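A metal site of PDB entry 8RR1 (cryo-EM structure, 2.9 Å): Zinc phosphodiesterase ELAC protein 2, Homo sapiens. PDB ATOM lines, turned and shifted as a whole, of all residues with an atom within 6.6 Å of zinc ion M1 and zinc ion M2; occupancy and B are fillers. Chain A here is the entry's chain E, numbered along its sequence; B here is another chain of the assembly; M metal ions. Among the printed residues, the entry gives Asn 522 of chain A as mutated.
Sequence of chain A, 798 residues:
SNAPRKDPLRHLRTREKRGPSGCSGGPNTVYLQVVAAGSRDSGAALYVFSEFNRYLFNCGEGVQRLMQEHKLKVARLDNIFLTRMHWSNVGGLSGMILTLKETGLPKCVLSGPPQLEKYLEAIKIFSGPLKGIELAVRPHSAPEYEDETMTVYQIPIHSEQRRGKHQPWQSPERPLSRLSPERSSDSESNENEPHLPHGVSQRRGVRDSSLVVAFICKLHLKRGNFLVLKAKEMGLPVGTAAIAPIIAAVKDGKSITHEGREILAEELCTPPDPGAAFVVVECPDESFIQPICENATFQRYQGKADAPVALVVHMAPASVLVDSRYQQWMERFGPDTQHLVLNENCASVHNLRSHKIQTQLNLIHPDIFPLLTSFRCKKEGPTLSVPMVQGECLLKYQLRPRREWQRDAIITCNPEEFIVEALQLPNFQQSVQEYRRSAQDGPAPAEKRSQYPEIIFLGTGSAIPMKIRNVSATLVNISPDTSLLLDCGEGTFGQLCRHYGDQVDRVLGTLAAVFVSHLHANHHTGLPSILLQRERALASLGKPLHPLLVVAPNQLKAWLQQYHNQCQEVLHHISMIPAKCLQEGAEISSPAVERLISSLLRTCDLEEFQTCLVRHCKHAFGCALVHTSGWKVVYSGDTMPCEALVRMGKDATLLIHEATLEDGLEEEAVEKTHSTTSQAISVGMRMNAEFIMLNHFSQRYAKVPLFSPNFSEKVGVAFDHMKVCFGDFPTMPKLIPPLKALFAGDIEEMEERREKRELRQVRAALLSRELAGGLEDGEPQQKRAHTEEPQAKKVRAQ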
ATOM      1  N   GLY A 461     -29.342  14.362  17.927  1.00  0.00           N
ATOM      2  CA  GLY A 461     -28.094  13.666  17.698  1.00  0.00           C
ATOM      3  C   GLY A 461     -28.230  12.206  18.090  1.00  0.00           C
ATOM      4  O   GLY A 461     -29.068  11.824  18.906  1.00  0.00           O
ATOM      5  N   SER A 462     -27.369  11.375  17.479  1.00  0.00           N
ATOM      6  CA  SER A 462     -27.634   9.938  17.511  1.00  0.00           C
ATOM      7  C   SER A 462     -27.114   9.241  18.753  1.00  0.00           C
ATOM      8  O   SER A 462     -27.890   8.918  19.664  1.00  0.00           O
ATOM      9  CB  SER A 462     -27.025   9.273  16.277  1.00  0.00           C
ATOM     10  OG  SER A 462     -25.655   9.612  16.146  1.00  0.00           O
ATOM     11  N   ALA A 463     -25.803   8.983  18.818  1.00  0.00           N
ATOM     12  CA  ALA A 463     -25.276   8.176  19.916  1.00  0.00           C
ATOM     13  C   ALA A 463     -24.723   8.995  21.078  1.00  0.00           C
ATOM     14  O   ALA A 463     -25.334   9.067  22.142  1.00  0.00           O
ATOM     15  CB  ALA A 463     -24.182   7.238  19.384  1.00  0.00           C
ATOM     16  N   SER A 472     -31.341  12.152  21.298  1.00  0.00           N
ATOM     17  CA  SER A 472     -32.629  12.384  20.664  1.00  0.00           C
ATOM     18  C   SER A 472     -33.700  12.730  21.691  1.00  0.00           C
ATOM     19  O   SER A 472     -33.711  12.218  22.816  1.00  0.00           O
ATOM     20  CB  SER A 472     -33.055  11.154  19.864  1.00  0.00           C
ATOM     21  OG  SER A 472     -32.978   9.973  20.659  1.00  0.00           O
ATOM     22  N   SER A 517     -39.171   4.542  22.091  1.00  0.00           N
ATOM     23  CA  SER A 517     -39.119   3.703  20.901  1.00  0.00           C
ATOM     24  C   SER A 517     -37.790   2.956  20.911  1.00  0.00           C
ATOM     25  O   SER A 517     -36.745   3.542  20.615  1.00  0.00           O
ATOM     26  CB  SER A 517     -39.284   4.541  19.640  1.00  0.00           C
ATOM     27  OG  SER A 517     -38.313   5.559  19.586  1.00  0.00           O
ATOM     28  N   HIS A 518     -37.844   1.670  21.272  1.00  0.00           N
ATOM     29  CA  HIS A 518     -36.706   0.747  21.264  1.00  0.00           C
ATOM     30  C   HIS A 518     -35.700   1.100  22.357  1.00  0.00           C
ATOM     31  O   HIS A 518     -35.415   2.275  22.598  1.00  0.00           O
ATOM     32  CB  HIS A 518     -36.064   0.677  19.867  1.00  0.00           C
ATOM     33  CG  HIS A 518     -34.856   1.544  19.687  1.00  0.00           C
ATOM     34  ND1 HIS A 518     -34.925   2.921  19.631  1.00  0.00           N
ATOM     35  CD2 HIS A 518     -33.546   1.227  19.503  1.00  0.00           C
ATOM     36  CE1 HIS A 518     -33.707   3.414  19.454  1.00  0.00           C
ATOM     37  NE2 HIS A 518     -32.861   2.404  19.373  1.00  0.00           N
ATOM     38  N   HIS A 520     -32.542   1.119  23.118  1.00  0.00           N
ATOM     39  CA  HIS A 520     -31.146   1.538  23.053  1.00  0.00           C
ATOM     40  C   HIS A 520     -30.869   2.598  24.116  1.00  0.00           C
ATOM     41  O   HIS A 520     -31.770   3.346  24.522  1.00  0.00           O
ATOM     42  CB  HIS A 520     -30.789   2.092  21.675  1.00  0.00           C
ATOM     43  CG  HIS A 520     -30.395   1.032  20.695  1.00  0.00           C
ATOM     44  ND1 HIS A 520     -30.174   1.300  19.358  1.00  0.00           N
ATOM     45  CD2 HIS A 520     -30.156  -0.289  20.856  1.00  0.00           C
ATOM     46  CE1 HIS A 520     -29.847   0.173  18.735  1.00  0.00           C
ATOM     47  NE2 HIS A 520     -29.816  -0.797  19.621  1.00  0.00           N
ATOM     48  N   ALA A 521     -29.628   2.661  24.563  1.00  0.00           N
ATOM     49  CA  ALA A 521     -29.217   3.722  25.469  1.00  0.00           C
ATOM     50  C   ALA A 521     -29.386   5.078  24.780  1.00  0.00           C
ATOM     51  O   ALA A 521     -29.539   5.179  23.567  1.00  0.00           O
ATOM     52  CB  ALA A 521     -27.775   3.534  25.911  1.00  0.00           C
ATOM     53  N   ASN A 522     -29.391   6.133  25.610  1.00  0.00           N
ATOM     54  CA  ASN A 522     -29.519   7.524  25.171  1.00  0.00           C
ATOM     55  C   ASN A 522     -30.848   7.785  24.486  1.00  0.00           C
ATOM     56  O   ASN A 522     -31.099   8.898  24.002  1.00  0.00           O
ATOM     57  CB  ASN A 522     -28.340   7.917  24.259  1.00  0.00           C
ATOM     58  CG  ASN A 522     -28.659   7.797  22.784  1.00  0.00           C
ATOM     59  OD1 ASN A 522     -29.071   8.769  22.143  1.00  0.00           O
ATOM     60  ND2 ASN A 522     -28.469   6.601  22.235  1.00  0.00           N
ATOM     61  N   HIS A 523     -31.736   6.786  24.453  1.00  0.00           N
ATOM     62  CA  HIS A 523     -33.113   6.987  24.050  1.00  0.00           C
ATOM     63  C   HIS A 523     -34.101   6.930  25.208  1.00  0.00           C
ATOM     64  O   HIS A 523     -35.228   7.407  25.058  1.00  0.00           O
ATOM     65  CB  HIS A 523     -33.532   5.926  23.014  1.00  0.00           C
ATOM     66  CG  HIS A 523     -33.178   6.283  21.601  1.00  0.00           C
ATOM     67  ND1 HIS A 523     -34.117   6.499  20.625  1.00  0.00           N
ATOM     68  CD2 HIS A 523     -31.969   6.479  21.005  1.00  0.00           C
ATOM     69  CE1 HIS A 523     -33.518   6.795  19.485  1.00  0.00           C
ATOM     70  NE2 HIS A 523     -32.211   6.791  19.688  1.00  0.00           N
ATOM     71  N   HIS A 616     -35.362  -1.976  12.923  1.00  0.00           N
ATOM     72  CA  HIS A 616     -34.104  -1.487  13.463  1.00  0.00           C
ATOM     73  C   HIS A 616     -33.432  -2.496  14.385  1.00  0.00           C
ATOM     74  O   HIS A 616     -32.262  -2.836  14.193  1.00  0.00           O
ATOM     75  CB  HIS A 616     -34.313  -0.167  14.211  1.00  0.00           C
ATOM     76  CG  HIS A 616     -33.132   0.267  15.028  1.00  0.00           C
ATOM     77  ND1 HIS A 616     -31.965   0.743  14.456  1.00  0.00           N
ATOM     78  CD2 HIS A 616     -32.944   0.304  16.363  1.00  0.00           C
ATOM     79  CE1 HIS A 616     -31.107   1.040  15.404  1.00  0.00           C
ATOM     80  NE2 HIS A 616     -31.667   0.783  16.570  1.00  0.00           N
ATOM     81  N   CYS A 617     -34.151  -2.985  15.399  1.00  0.00           N
ATOM     82  CA  CYS A 617     -33.638  -3.969  16.330  1.00  0.00           C
ATOM     83  C   CYS A 617     -34.804  -4.829  16.789  1.00  0.00           C
ATOM     84  O   CYS A 617     -35.885  -4.813  16.200  1.00  0.00           O
ATOM     85  CB  CYS A 617     -32.915  -3.283  17.497  1.00  0.00           C
ATOM     86  SG  CYS A 617     -31.168  -2.921  17.205  1.00  0.00           S
ATOM     87  N   ASP A 638     -35.416   5.207  15.355  1.00  0.00           N
ATOM     88  CA  ASP A 638     -34.388   4.393  14.722  1.00  0.00           C
ATOM     89  C   ASP A 638     -35.039   3.306  13.892  1.00  0.00           C
ATOM     90  O   ASP A 638     -35.849   2.522  14.407  1.00  0.00           O
ATOM     91  CB  ASP A 638     -33.462   3.784  15.784  1.00  0.00           C
ATOM     92  CG  ASP A 638     -32.684   4.837  16.543  1.00  0.00           C
ATOM     93  OD1 ASP A 638     -32.987   6.034  16.377  1.00  0.00           O
ATOM     94  OD2 ASP A 638     -31.770   4.469  17.307  1.00  0.00           O
ATOM     95  N   THR A 639     -34.723   3.258  12.598  1.00  0.00           N
ATOM     96  CA  THR A 639     -35.358   2.311  11.693  1.00  0.00           C
ATOM     97  C   THR A 639     -34.573   2.252  10.391  1.00  0.00           C
ATOM     98  O   THR A 639     -33.564   2.932  10.214  1.00  0.00           O
ATOM     99  CB  THR A 639     -36.819   2.669  11.406  1.00  0.00           C
ATOM    100  OG1 THR A 639     -37.381   1.705  10.514  1.00  0.00           O
ATOM    101  CG2 THR A 639     -36.901   4.033  10.753  1.00  0.00           C
ATOM    102  N   GLU A 658     -35.696   9.138  10.822  1.00  0.00           N
ATOM    103  CA  GLU A 658     -34.269   9.036  11.071  1.00  0.00           C
ATOM    104  C   GLU A 658     -33.463   9.308   9.802  1.00  0.00           C
ATOM    105  O   GLU A 658     -33.805   8.816   8.725  1.00  0.00           O
ATOM    106  CB  GLU A 658     -33.934   7.648  11.623  1.00  0.00           C
ATOM    107  CG  GLU A 658     -32.464   7.310  11.603  1.00  0.00           C
ATOM    108  CD  GLU A 658     -32.215   5.847  11.312  1.00  0.00           C
ATOM    109  OE1 GLU A 658     -32.636   4.997  12.110  1.00  0.00           O
ATOM    110  OE2 GLU A 658     -31.602   5.552  10.264  1.00  0.00           O
ATOM    111  N   THR A 673     -28.272  -1.124  10.587  1.00  0.00           N
ATOM    112  CA  THR A 673     -29.728  -1.002  10.676  1.00  0.00           C
ATOM    113  C   THR A 673     -30.140   0.467  10.882  1.00  0.00           C
ATOM    114  O   THR A 673     -30.712   0.848  11.897  1.00  0.00           O
ATOM    115  CB  THR A 673     -30.288  -1.884  11.790  1.00  0.00           C
ATOM    116  OG1 THR A 673     -29.959  -1.339  13.077  1.00  0.00           O
ATOM    117  CG2 THR A 673     -29.734  -3.302  11.685  1.00  0.00           C
ATOM    118  N   HIS A 674     -29.824   1.274   9.882  1.00  0.00           N
ATOM    119  CA  HIS A 674     -30.170   2.689   9.879  1.00  0.00           C
ATOM    120  C   HIS A 674     -30.526   3.117   8.459  1.00  0.00           C
ATOM    121  O   HIS A 674     -30.243   2.415   7.489  1.00  0.00           O
ATOM    122  CB  HIS A 674     -29.033   3.545  10.433  1.00  0.00           C
ATOM    123  CG  HIS A 674     -29.048   3.680  11.932  1.00  0.00           C
ATOM    124  ND1 HIS A 674     -29.603   4.760  12.575  1.00  0.00           N
ATOM    125  CD2 HIS A 674     -28.570   2.865  12.892  1.00  0.00           C
ATOM    126  CE1 HIS A 674     -29.475   4.600  13.880  1.00  0.00           C
ATOM    127  NE2 HIS A 674     -28.851   3.462  14.105  1.00  0.00           N
ATOM    128  N   HIS A 696     -31.937  12.564  14.394  1.00  0.00           N
ATOM    129  CA  HIS A 696     -31.072  11.436  14.744  1.00  0.00           C
ATOM    130  C   HIS A 696     -29.809  11.409  13.879  1.00  0.00           C
ATOM    131  O   HIS A 696     -29.363  10.355  13.431  1.00  0.00           O
ATOM    132  CB  HIS A 696     -31.825  10.110  14.653  1.00  0.00           C
ATOM    133  CG  HIS A 696     -31.328   9.073  15.605  1.00  0.00           C
ATOM    134  ND1 HIS A 696     -30.265   8.249  15.322  1.00  0.00           N
ATOM    135  CD2 HIS A 696     -31.764   8.720  16.839  1.00  0.00           C
ATOM    136  CE1 HIS A 696     -30.058   7.432  16.339  1.00  0.00           C
ATOM    137  NE2 HIS A 696     -30.948   7.701  17.277  1.00  0.00           N
ATOM    138  P     A B  66     -19.204   3.137  16.600  1.00  0.00           P
ATOM    139  OP1   A B  66     -19.446   2.065  15.565  1.00  0.00           O
ATOM    140  OP2   A B  66     -20.005   4.407  16.376  1.00  0.00           O
ATOM    141  O5'   A B  66     -19.632   2.525  18.040  1.00  0.00           O
ATOM    142  C5'   A B  66     -20.763   3.085  18.782  1.00  0.00           C
ATOM    143  C4'   A B  66     -22.053   2.752  18.086  1.00  0.00           C
ATOM    144  O4'   A B  66     -21.816   1.753  17.056  1.00  0.00           O
ATOM    145  C3'   A B  66     -23.168   2.111  18.925  1.00  0.00           C
ATOM    146  O3'   A B  66     -23.894   3.002  19.764  1.00  0.00           O
ATOM    147  C2'   A B  66     -24.015   1.528  17.790  1.00  0.00           C
ATOM    148  O2'   A B  66     -24.719   2.504  17.057  1.00  0.00           O
ATOM    149  C1'   A B  66     -22.907   0.877  16.969  1.00  0.00           C
ATOM    150  N9    A B  66     -22.529  -0.423  17.511  1.00  0.00           N
ATOM    151  C8    A B  66     -23.398  -1.460  17.769  1.00  0.00           C
ATOM    152  N7    A B  66     -22.811  -2.525  18.242  1.00  0.00           N
ATOM    153  C5    A B  66     -21.466  -2.177  18.301  1.00  0.00           C
ATOM    154  C6    A B  66     -20.339  -2.889  18.720  1.00  0.00           C
ATOM    155  N6    A B  66     -20.377  -4.145  19.176  1.00  0.00           N
ATOM    156  N1    A B  66     -19.140  -2.260  18.641  1.00  0.00           N
ATOM    157  C2    A B  66     -19.110  -1.006  18.191  1.00  0.00           C
ATOM    158  N3    A B  66     -20.107  -0.241  17.770  1.00  0.00           N
ATOM    159  C4    A B  66     -21.277  -0.896  17.833  1.00  0.00           C
ATOM    160  P     G B  67     -25.266   2.541  20.466  1.00  0.00           P
ATOM    161  OP1   G B  67     -26.445   2.874  19.574  1.00  0.00           O
ATOM    162  OP2   G B  67     -25.425   3.052  21.881  1.00  0.00           O
ATOM    163  O5'   G B  67     -25.164   0.926  20.545  1.00  0.00           O
ATOM    164  C5'   G B  67     -25.544   0.236  21.766  1.00  0.00           C
ATOM    165  C4'   G B  67     -25.172  -1.223  21.661  1.00  0.00           C
ATOM    166  O4'   G B  67     -23.781  -1.308  21.250  1.00  0.00           O
ATOM    167  C3'   G B  67     -25.258  -2.031  22.958  1.00  0.00           C
ATOM    168  O3'   G B  67     -25.438  -3.437  22.787  1.00  0.00           O
ATOM    169  C2'   G B  67     -23.861  -1.798  23.561  1.00  0.00           C
ATOM    170  O2'   G B  67     -23.461  -2.826  24.432  1.00  0.00           O
ATOM    171  C1'   G B  67     -22.990  -1.787  22.321  1.00  0.00           C
ATOM    172  N9    G B  67     -21.824  -0.925  22.457  1.00  0.00           N
ATOM    173  C8    G B  67     -21.739   0.411  22.163  1.00  0.00           C
ATOM    174  N7    G B  67     -20.559   0.916  22.395  1.00  0.00           N
ATOM    175  C5    G B  67     -19.814  -0.152  22.880  1.00  0.00           C
ATOM    176  C6    G B  67     -18.474  -0.206  23.306  1.00  0.00           C
ATOM    177  O6    G B  67     -17.638   0.714  23.342  1.00  0.00           O
ATOM    178  N1    G B  67     -18.117  -1.478  23.721  1.00  0.00           N
ATOM    179  C2    G B  67     -18.952  -2.567  23.729  1.00  0.00           C
ATOM    180  N2    G B  67     -18.416  -3.725  24.169  1.00  0.00           N
ATOM    181  N3    G B  67     -20.220  -2.529  23.330  1.00  0.00           N
ATOM    182  C4    G B  67     -20.580  -1.288  22.923  1.00  0.00           C
HETATM  183 ZN    ZN M   1     -31.190   2.653  17.818  1.00  0.00          ZN
HETATM  184 ZN    ZN M   2     -30.602   5.738  18.430  1.00  0.00          ZN
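Along chain A the residues within 4 Å of zinc ion M1 span positions 518 to 638. The nearest printed residue that does not touch zinc ion M1 is His 674 (4.5 Å).
Zinc ion M1 is bound by the side-chain carboxylate of Asp 638 (2.0 Å), a ring nitrogen (ND1) of His 520 (2.3 Å), a ring nitrogen (NE2) of His 518 (2.3 Å) and a ring nitrogen (NE2) of His 616 (2.3 Å).
The side-chain sulfur of Cys 617 sits at hydrogen-bond distance from a ring nitrogen (NE2) of His 520 (3.5 Å). The side-chain hydroxyl (OG) of Ser 472 sits close to a ring nitrogen (NE2) of His 523 (3.4 Å). A ring nitrogen (NE2) of His 616 lies close to the side-chain sulfur of Cys 617, at 3.8 Å. The backbone carbonyl oxygen of Thr 673 is in hydrogen-bond range of a ring nitrogen (ND1) of His 616 (2.9 Å).
Zinc ion M2 is bound by the side-chain carboxylate of Asp 638, a ring nitrogen (NE2) of His 523 and a ring nitrogen (NE2) of His 696. Zinc ion M2 has three donor atoms within binding distance.
Of the 20 residues printed, 3 come within 4 Å of zinc ion M2. The nearest printed residue that does not touch zinc ion M2 is His 518 (4.01 Å).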
